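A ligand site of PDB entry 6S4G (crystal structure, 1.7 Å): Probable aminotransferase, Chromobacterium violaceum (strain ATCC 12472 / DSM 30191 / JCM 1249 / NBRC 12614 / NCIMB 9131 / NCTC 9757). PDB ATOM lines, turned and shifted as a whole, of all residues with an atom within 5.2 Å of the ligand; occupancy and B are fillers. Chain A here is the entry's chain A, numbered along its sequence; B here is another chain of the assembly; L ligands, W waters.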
ATOM      1  N   LEU A  65     -21.712   8.574  10.249  1.00  0.00           N
ATOM      2  CA  LEU A  65     -20.802   9.452   9.498  1.00  0.00           C
ATOM      3  C   LEU A  65     -20.003   8.545   8.552  1.00  0.00           C
ATOM      4  O   LEU A  65     -18.833   8.267   8.832  1.00  0.00           O
ATOM      5  CB  LEU A  65     -19.954  10.208  10.526  1.00  0.00           C
ATOM      6  CG  LEU A  65     -19.103  11.345   9.955  1.00  0.00           C
ATOM      7  CD1 LEU A  65     -19.917  12.354   9.163  1.00  0.00           C
ATOM      8  CD2 LEU A  65     -18.323  12.046  11.059  1.00  0.00           C
ATOM      9  N   TRP A  66     -20.658   8.095   7.484  1.00  0.00           N
ATOM     10  CA  TRP A  66     -20.114   7.174   6.453  1.00  0.00           C
ATOM     11  C   TRP A  66     -19.644   5.837   7.072  1.00  0.00           C
ATOM     12  O   TRP A  66     -18.742   5.234   6.500  1.00  0.00           O
ATOM     13  CB  TRP A  66     -18.855   7.804   5.799  1.00  0.00           C
ATOM     14  CG  TRP A  66     -18.831   9.254   5.454  1.00  0.00           C
ATOM     15  CD1 TRP A  66     -18.475  10.283   6.274  1.00  0.00           C
ATOM     16  CD2 TRP A  66     -18.969   9.840   4.148  1.00  0.00           C
ATOM     17  NE1 TRP A  66     -18.445  11.460   5.587  1.00  0.00           N
ATOM     18  CE2 TRP A  66     -18.751  11.214   4.282  1.00  0.00           C
ATOM     19  CE3 TRP A  66     -19.299   9.327   2.896  1.00  0.00           C
ATOM     20  CZ2 TRP A  66     -18.814  12.095   3.214  1.00  0.00           C
ATOM     21  CZ3 TRP A  66     -19.325  10.181   1.826  1.00  0.00           C
ATOM     22  CH2 TRP A  66     -19.122  11.549   2.004  1.00  0.00           C
ATOM     23  N   SER A 125      -8.753   5.630  15.852  1.00  0.00           N
ATOM     24  CA  SER A 125      -9.465   6.541  14.922  1.00  0.00           C
ATOM     25  C   SER A 125      -8.777   6.528  13.559  1.00  0.00           C
ATOM     26  O   SER A 125      -7.611   6.136  13.427  1.00  0.00           O
ATOM     27  CB  SER A 125      -9.494   7.962  15.467  1.00  0.00           C
ATOM     28  OG  SER A 125      -8.179   8.489  15.511  1.00  0.00           O
ATOM     29  N   GLY A 126      -9.499   6.981  12.563  1.00  0.00           N
ATOM     30  CA  GLY A 126      -8.895   7.258  11.229  1.00  0.00           C
ATOM     31  C   GLY A 126      -7.764   8.262  11.305  1.00  0.00           C
ATOM     32  O   GLY A 126      -6.779   8.076  10.602  1.00  0.00           O
ATOM     33  N   SER A 127      -7.914   9.296  12.129  1.00  0.00           N
ATOM     34  CA  SER A 127      -6.915  10.383  12.285  1.00  0.00           C
ATOM     35  C   SER A 127      -5.609   9.762  12.833  1.00  0.00           C
ATOM     36  O   SER A 127      -4.515  10.094  12.356  1.00  0.00           O
ATOM     37  CB  SER A 127      -7.449  11.486  13.140  1.00  0.00           C
ATOM     38  OG  SER A 127      -8.579  12.097  12.551  1.00  0.00           O
ATOM     39  N   GLU A 128      -5.729   8.921  13.863  1.00  0.00           N
ATOM     40  CA  GLU A 128      -4.545   8.259  14.451  1.00  0.00           C
ATOM     41  C   GLU A 128      -3.933   7.322  13.418  1.00  0.00           C
ATOM     42  O   GLU A 128      -2.702   7.233  13.359  1.00  0.00           O
ATOM     43  CB  GLU A 128      -4.910   7.532  15.761  1.00  0.00           C
ATOM     44  CG  GLU A 128      -5.113   8.431  16.933  1.00  0.00           C
ATOM     45  CD  GLU A 128      -5.630   7.580  18.125  1.00  0.00           C
ATOM     46  OE1 GLU A 128      -5.802   6.381  17.948  1.00  0.00           O
ATOM     47  OE2 GLU A 128      -5.826   8.092  19.229  1.00  0.00           O
ATOM     48  N   VAL A 130      -3.848   7.770  10.230  1.00  0.00           N
ATOM     49  CA  VAL A 130      -3.101   8.660   9.296  1.00  0.00           C
ATOM     50  C   VAL A 130      -1.798   9.114   9.958  1.00  0.00           C
ATOM     51  O   VAL A 130      -0.755   9.012   9.308  1.00  0.00           O
ATOM     52  CB  VAL A 130      -3.967   9.808   8.776  1.00  0.00           C
ATOM     53  CG1 VAL A 130      -3.094  10.844   8.060  1.00  0.00           C
ATOM     54  CG2 VAL A 130      -5.098   9.282   7.858  1.00  0.00           C
ATOM     55  N   TYR A 159      -9.296  14.835   2.447  1.00  0.00           N
ATOM     56  CA  TYR A 159      -9.498  14.811   3.919  1.00  0.00           C
ATOM     57  C   TYR A 159      -8.844  13.564   4.464  1.00  0.00           C
ATOM     58  O   TYR A 159      -9.153  12.490   4.057  1.00  0.00           O
ATOM     59  CB  TYR A 159     -11.000  14.872   4.261  1.00  0.00           C
ATOM     60  CG  TYR A 159     -11.190  15.025   5.744  1.00  0.00           C
ATOM     61  CD1 TYR A 159     -11.014  16.227   6.348  1.00  0.00           C
ATOM     62  CD2 TYR A 159     -11.481  13.938   6.534  1.00  0.00           C
ATOM     63  CE1 TYR A 159     -11.086  16.367   7.729  1.00  0.00           C
ATOM     64  CE2 TYR A 159     -11.575  14.059   7.921  1.00  0.00           C
ATOM     65  CZ  TYR A 159     -11.397  15.274   8.528  1.00  0.00           C
ATOM     66  OH  TYR A 159     -11.481  15.402   9.908  1.00  0.00           O
ATOM     67  N   HIS A 160      -7.950  13.736   5.439  1.00  0.00           N
ATOM     68  CA  HIS A 160      -7.178  12.642   6.052  1.00  0.00           C
ATOM     69  C   HIS A 160      -7.196  12.821   7.580  1.00  0.00           C
ATOM     70  O   HIS A 160      -6.224  12.358   8.237  1.00  0.00           O
ATOM     71  CB  HIS A 160      -5.740  12.622   5.486  1.00  0.00           C
ATOM     72  CG  HIS A 160      -5.738  12.285   4.046  1.00  0.00           C
ATOM     73  ND1 HIS A 160      -5.505  13.209   3.034  1.00  0.00           N
ATOM     74  CD2 HIS A 160      -6.188  11.190   3.425  1.00  0.00           C
ATOM     75  CE1 HIS A 160      -5.681  12.624   1.861  1.00  0.00           C
ATOM     76  NE2 HIS A 160      -6.065  11.363   2.077  1.00  0.00           N
ATOM     77  N   GLY A 161      -8.271  13.393   8.100  1.00  0.00           N
ATOM     78  CA  GLY A 161      -8.469  13.421   9.559  1.00  0.00           C
ATOM     79  C   GLY A 161      -8.065  14.733  10.176  1.00  0.00           C
ATOM     80  O   GLY A 161      -7.844  15.743   9.465  1.00  0.00           O
ATOM     81  N   SER A 162      -7.987  14.730  11.514  1.00  0.00           N
ATOM     82  CA  SER A 162      -8.056  15.994  12.286  1.00  0.00           C
ATOM     83  C   SER A 162      -6.952  16.041  13.353  1.00  0.00           C
ATOM     84  O   SER A 162      -6.980  16.966  14.200  1.00  0.00           O
ATOM     85  CB  SER A 162      -9.392  16.142  12.903  1.00  0.00           C
ATOM     86  OG  SER A 162      -9.462  17.400  13.508  1.00  0.00           O
ATOM     87  N   GLU A 232      -7.487   9.392  -0.841  1.00  0.00           N
ATOM     88  CA  GLU A 232      -8.791   8.654  -0.768  1.00  0.00           C
ATOM     89  C   GLU A 232      -9.161   8.137  -2.169  1.00  0.00           C
ATOM     90  O   GLU A 232      -9.080   8.912  -3.121  1.00  0.00           O
ATOM     91  CB  GLU A 232      -9.895   9.602  -0.340  1.00  0.00           C
ATOM     92  CG  GLU A 232      -9.677  10.248   1.029  1.00  0.00           C
ATOM     93  CD  GLU A 232     -10.547  11.485   1.113  1.00  0.00           C
ATOM     94  OE1 GLU A 232     -11.742  11.335   1.585  1.00  0.00           O
ATOM     95  OE2 GLU A 232     -10.109  12.600   0.739  1.00  0.00           O
ATOM     96  N   ASP A 265      -6.088   6.070   1.485  1.00  0.00           N
ATOM     97  CA  ASP A 265      -6.855   6.342   2.710  1.00  0.00           C
ATOM     98  C   ASP A 265      -8.242   5.706   2.522  1.00  0.00           C
ATOM     99  O   ASP A 265      -9.059   6.268   1.803  1.00  0.00           O
ATOM    100  CB  ASP A 265      -6.965   7.847   3.019  1.00  0.00           C
ATOM    101  CG  ASP A 265      -7.545   8.073   4.398  1.00  0.00           C
ATOM    102  OD1 ASP A 265      -8.132   7.116   4.976  1.00  0.00           O
ATOM    103  OD2 ASP A 265      -7.450   9.217   4.898  1.00  0.00           O
ATOM    104  N   VAL A 267     -10.391   5.077   4.883  1.00  0.00           N
ATOM    105  CA  VAL A 267     -11.228   5.281   6.095  1.00  0.00           C
ATOM    106  C   VAL A 267     -12.729   5.269   5.714  1.00  0.00           C
ATOM    107  O   VAL A 267     -13.509   4.607   6.413  1.00  0.00           O
ATOM    108  CB  VAL A 267     -10.772   6.489   6.896  1.00  0.00           C
ATOM    109  CG1 VAL A 267     -11.868   6.875   7.903  1.00  0.00           C
ATOM    110  CG2 VAL A 267      -9.443   6.156   7.599  1.00  0.00           C
ATOM    111  N   ILE A 268     -13.106   5.801   4.567  1.00  0.00           N
ATOM    112  CA  ILE A 268     -14.538   5.738   4.132  1.00  0.00           C
ATOM    113  C   ILE A 268     -14.746   4.577   3.162  1.00  0.00           C
ATOM    114  O   ILE A 268     -15.772   3.863   3.334  1.00  0.00           O
ATOM    115  CB  ILE A 268     -14.959   7.077   3.501  1.00  0.00           C
ATOM    116  CG1 ILE A 268     -15.240   8.147   4.548  1.00  0.00           C
ATOM    117  CG2 ILE A 268     -16.166   6.917   2.618  1.00  0.00           C
ATOM    118  CD1 ILE A 268     -15.395   9.516   3.902  1.00  0.00           C
ATOM    119  N   ALA A 293     -10.743   2.909   9.300  1.00  0.00           N
ATOM    120  CA  ALA A 293     -11.504   3.038  10.548  1.00  0.00           C
ATOM    121  C   ALA A 293     -12.968   2.852  10.216  1.00  0.00           C
ATOM    122  O   ALA A 293     -13.251   1.964   9.358  1.00  0.00           O
ATOM    123  CB  ALA A 293     -11.141   4.385  11.126  1.00  0.00           C
ATOM    124  N   LYS A 294     -13.871   3.675  10.737  1.00  0.00           N
ATOM    125  CA  LYS A 294     -15.312   3.672  10.337  1.00  0.00           C
ATOM    126  C   LYS A 294     -15.901   2.265  10.191  1.00  0.00           C
ATOM    127  O   LYS A 294     -16.269   1.647  11.218  1.00  0.00           O
ATOM    128  CB  LYS A 294     -15.439   4.559   9.080  1.00  0.00           C
ATOM    129  CG  LYS A 294     -15.241   6.058   9.342  1.00  0.00           C
ATOM    130  CD  LYS A 294     -15.738   6.833   8.153  1.00  0.00           C
ATOM    131  CE  LYS A 294     -15.375   8.299   8.145  1.00  0.00           C
ATOM    132  NZ  LYS A 294     -16.142   9.102   9.119  1.00  0.00           N
ATOM    133  N   GLU B 128      -4.970  12.186  21.009  1.00  0.00           N
ATOM    134  CA  GLU B 128      -5.887  13.057  20.260  1.00  0.00           C
ATOM    135  C   GLU B 128      -6.252  14.278  21.134  1.00  0.00           C
ATOM    136  O   GLU B 128      -6.384  15.385  20.602  1.00  0.00           O
ATOM    137  CB  GLU B 128      -7.125  12.315  19.818  1.00  0.00           C
ATOM    138  CG  GLU B 128      -6.925  11.369  18.666  1.00  0.00           C
ATOM    139  CD  GLU B 128      -8.225  10.560  18.443  1.00  0.00           C
ATOM    140  OE1 GLU B 128      -9.161  10.766  19.196  1.00  0.00           O
ATOM    141  OE2 GLU B 128      -8.265   9.684  17.576  1.00  0.00           O
ATOM    142  N   GLY B 325     -11.988  17.789  15.004  1.00  0.00           N
ATOM    143  CA  GLY B 325     -12.655  16.725  15.759  1.00  0.00           C
ATOM    144  C   GLY B 325     -12.608  15.389  15.040  1.00  0.00           C
ATOM    145  O   GLY B 325     -12.134  15.295  13.901  1.00  0.00           O
ATOM    146  N   PHE B 326     -13.092  14.361  15.695  1.00  0.00           N
ATOM    147  CA  PHE B 326     -12.954  12.935  15.290  1.00  0.00           C
ATOM    148  C   PHE B 326     -14.342  12.328  15.143  1.00  0.00           C
ATOM    149  O   PHE B 326     -15.258  12.697  15.904  1.00  0.00           O
ATOM    150  CB  PHE B 326     -12.083  12.221  16.335  1.00  0.00           C
ATOM    151  CG  PHE B 326     -10.796  12.976  16.586  1.00  0.00           C
ATOM    152  CD1 PHE B 326      -9.765  12.895  15.666  1.00  0.00           C
ATOM    153  CD2 PHE B 326     -10.621  13.797  17.696  1.00  0.00           C
ATOM    154  CE1 PHE B 326      -8.586  13.634  15.802  1.00  0.00           C
ATOM    155  CE2 PHE B 326      -9.459  14.553  17.837  1.00  0.00           C
ATOM    156  CZ  PHE B 326      -8.424  14.454  16.892  1.00  0.00           C
ATOM    157  N   THR B 327     -14.510  11.466  14.133  1.00  0.00           N
ATOM    158  CA  THR B 327     -15.780  10.749  13.902  1.00  0.00           C
ATOM    159  C   THR B 327     -16.381  10.248  15.229  1.00  0.00           C
ATOM    160  O   THR B 327     -17.601  10.380  15.403  1.00  0.00           O
ATOM    161  CB  THR B 327     -15.573   9.547  12.961  1.00  0.00           C
ATOM    162  OG1 THR B 327     -15.023  10.031  11.730  1.00  0.00           O
ATOM    163  CG2 THR B 327     -16.841   8.793  12.694  1.00  0.00           C
ATOM    164  N   TYR B 328     -15.590   9.605  16.058  1.00  0.00           N
ATOM    165  CA  TYR B 328     -16.048   8.933  17.300  1.00  0.00           C
ATOM    166  C   TYR B 328     -15.999   9.896  18.487  1.00  0.00           C
ATOM    167  O   TYR B 328     -16.258   9.396  19.620  1.00  0.00           O
ATOM    168  CB  TYR B 328     -15.242   7.651  17.555  1.00  0.00           C
ATOM    169  CG  TYR B 328     -15.337   6.669  16.427  1.00  0.00           C
ATOM    170  CD1 TYR B 328     -16.541   6.505  15.732  1.00  0.00           C
ATOM    171  CD2 TYR B 328     -14.218   5.927  16.015  1.00  0.00           C
ATOM    172  CE1 TYR B 328     -16.638   5.622  14.659  1.00  0.00           C
ATOM    173  CE2 TYR B 328     -14.336   5.006  14.974  1.00  0.00           C
ATOM    174  CZ  TYR B 328     -15.553   4.816  14.347  1.00  0.00           C
ATOM    175  OH  TYR B 328     -15.646   3.934  13.310  1.00  0.00           O
HETATM  176  N1  LIG L   1      -9.524   9.803   6.487  1.00  0.00           N
HETATM  177  C1  LIG L   1     -10.687   9.936   5.838  1.00  0.00           C
HETATM  178  C2  LIG L   1     -10.698   9.613   4.365  1.00  0.00           C
HETATM  179  C3  LIG L   1     -11.870  10.328   6.551  1.00  0.00           C
HETATM  180  O1  LIG L   1     -13.104  10.518   5.927  1.00  0.00           O
HETATM  181  C4  LIG L   1     -11.777  10.559   7.947  1.00  0.00           C
HETATM  182  C5  LIG L   1     -12.981  10.982   8.791  1.00  0.00           C
HETATM  183  N2  LIG L   1     -14.273  11.271   8.098  1.00  0.00           N
HETATM  184  C6  LIG L   1     -10.539  10.406   8.570  1.00  0.00           C
HETATM  185  C7  LIG L   1      -9.455   9.982   7.825  1.00  0.00           C
HETATM  186  C8  LIG L   1     -10.440  10.607  10.046  1.00  0.00           C
HETATM  187  O2  LIG L   1     -11.084   9.506  10.784  1.00  0.00           O
HETATM  188  P1  LIG L   1     -11.445   9.867  12.332  1.00  0.00           P
HETATM  189  O3  LIG L   1     -10.255  10.380  13.161  1.00  0.00           O
HETATM  190  O4  LIG L   1     -12.552  10.951  12.200  1.00  0.00           O
HETATM  191  O5  LIG L   1     -11.972   8.469  12.819  1.00  0.00           O
HETATM  192  O   HOH W   1     -12.090  13.534  11.630  1.00  0.00           O
HETATM  193  O   HOH W   2     -13.188  12.122   3.704  1.00  0.00           O
HETATM  194  O   HOH W   3     -13.532   6.444  12.301  1.00  0.00           O
HETATM  195  O   HOH W   4     -12.860   8.729  15.343  1.00  0.00           O
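The backbone NH (N) of Ser 127 sits at hydrogen-bond distance from an oxygen (O3) of the ligand, at 2.8 Å.
The side-chain hydroxyl (OG) of Ser 127 sits at hydrogen-bond distance from an oxygen (O3) of the ligand (2.5 Å).
OD2 of Asp 265 lies within hydrogen-bond range of N1 of the ligand (2.7 Å).
N of Thr 327 of chain B lies within hydrogen-bond range of O4 of the ligand (2.8 Å).
OG1 of Thr 327 of chain B sits at hydrogen-bond distance from O4 of the ligand, 2.7 Å away.
O5 of the ligand lies within hydrogen-bond range of N of Gly 126 (2.9 Å).
The side-chain amino group (NZ) of Lys 294 lies close to a nitrogen (N2) of the ligand (3.0 Å).
Water W3 lies within hydrogen-bond range of an oxygen (O5) of the ligand (2.6 Å), the backbone NH (N) of Lys 294 (3.2 Å) and the side-chain hydroxyl (OH) of Tyr 328 of chain B (3.4 Å).
Water W1 lies within hydrogen-bond range of the side-chain hydroxyl of Tyr 159, an oxygen (O4) of the ligand and the backbone carbonyl oxygen of Gly 325 of chain B.
Water W4 lies within hydrogen-bond range of an oxygen (O5) of the ligand (2.7 Å), the backbone NH (N) of Tyr 328 of chain B (3.0 Å) and the backbone NH (N) of Thr 327 of chain B (3.4 Å).
Water W2 lies within hydrogen-bond range of the side-chain carboxylate (OE1) of Glu 232 (2.7 Å) and an oxygen (O1) of the ligand (2.7 Å).
N of Ser 127 lies close to OG of Ser 125, 3.5 Å away.
The side-chain hydroxyl (OG) of Ser 127 lies within hydrogen-bond range of the backbone NH (N) of Ser 162.
OD1 of Asp 265 is in hydrogen-bond range of N of Val 267 (3.0 Å).
The side-chain hydroxyl (OG1) of Thr 327 of chain B lies within hydrogen-bond range of the side-chain amino group (NZ) of Lys 294, at 3.0 Å.
The backbone NH of Lys 294 sits close to the side-chain hydroxyl of Tyr 328 of chain B, at 3.1 Å.
The backbone carbonyl oxygen (O) of Leu 65 sits at hydrogen-bond distance from the side-chain amino group (NZ) of Lys 294, at 2.8 Å.
N of Tyr 159 lies within hydrogen-bond range of OE2 of Glu 232, 2.9 Å away.
The side-chain hydroxyl (OG) of Ser 125 sits at hydrogen-bond distance from the backbone NH (N) of Glu 128 of chain A, at 3.0 Å.
Residues that only touch the ligand: Ser 125, Tyr 159, His 160, Gly 161, Glu 232, Val 267, Ile 268 and Phe 326 of chain B.
13 residues have an atom within 4 Å of the ligand: Ser 125, Gly 126, Ser 127, Tyr 159, His 160, Gly 161, Glu 232, Asp 265, Val 267, Ile 268, Lys 294, Phe 326 of chain B and Thr 327 of chain B.
The nearest printed residue that does not touch the ligand is Val 130 (4.4 Å).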
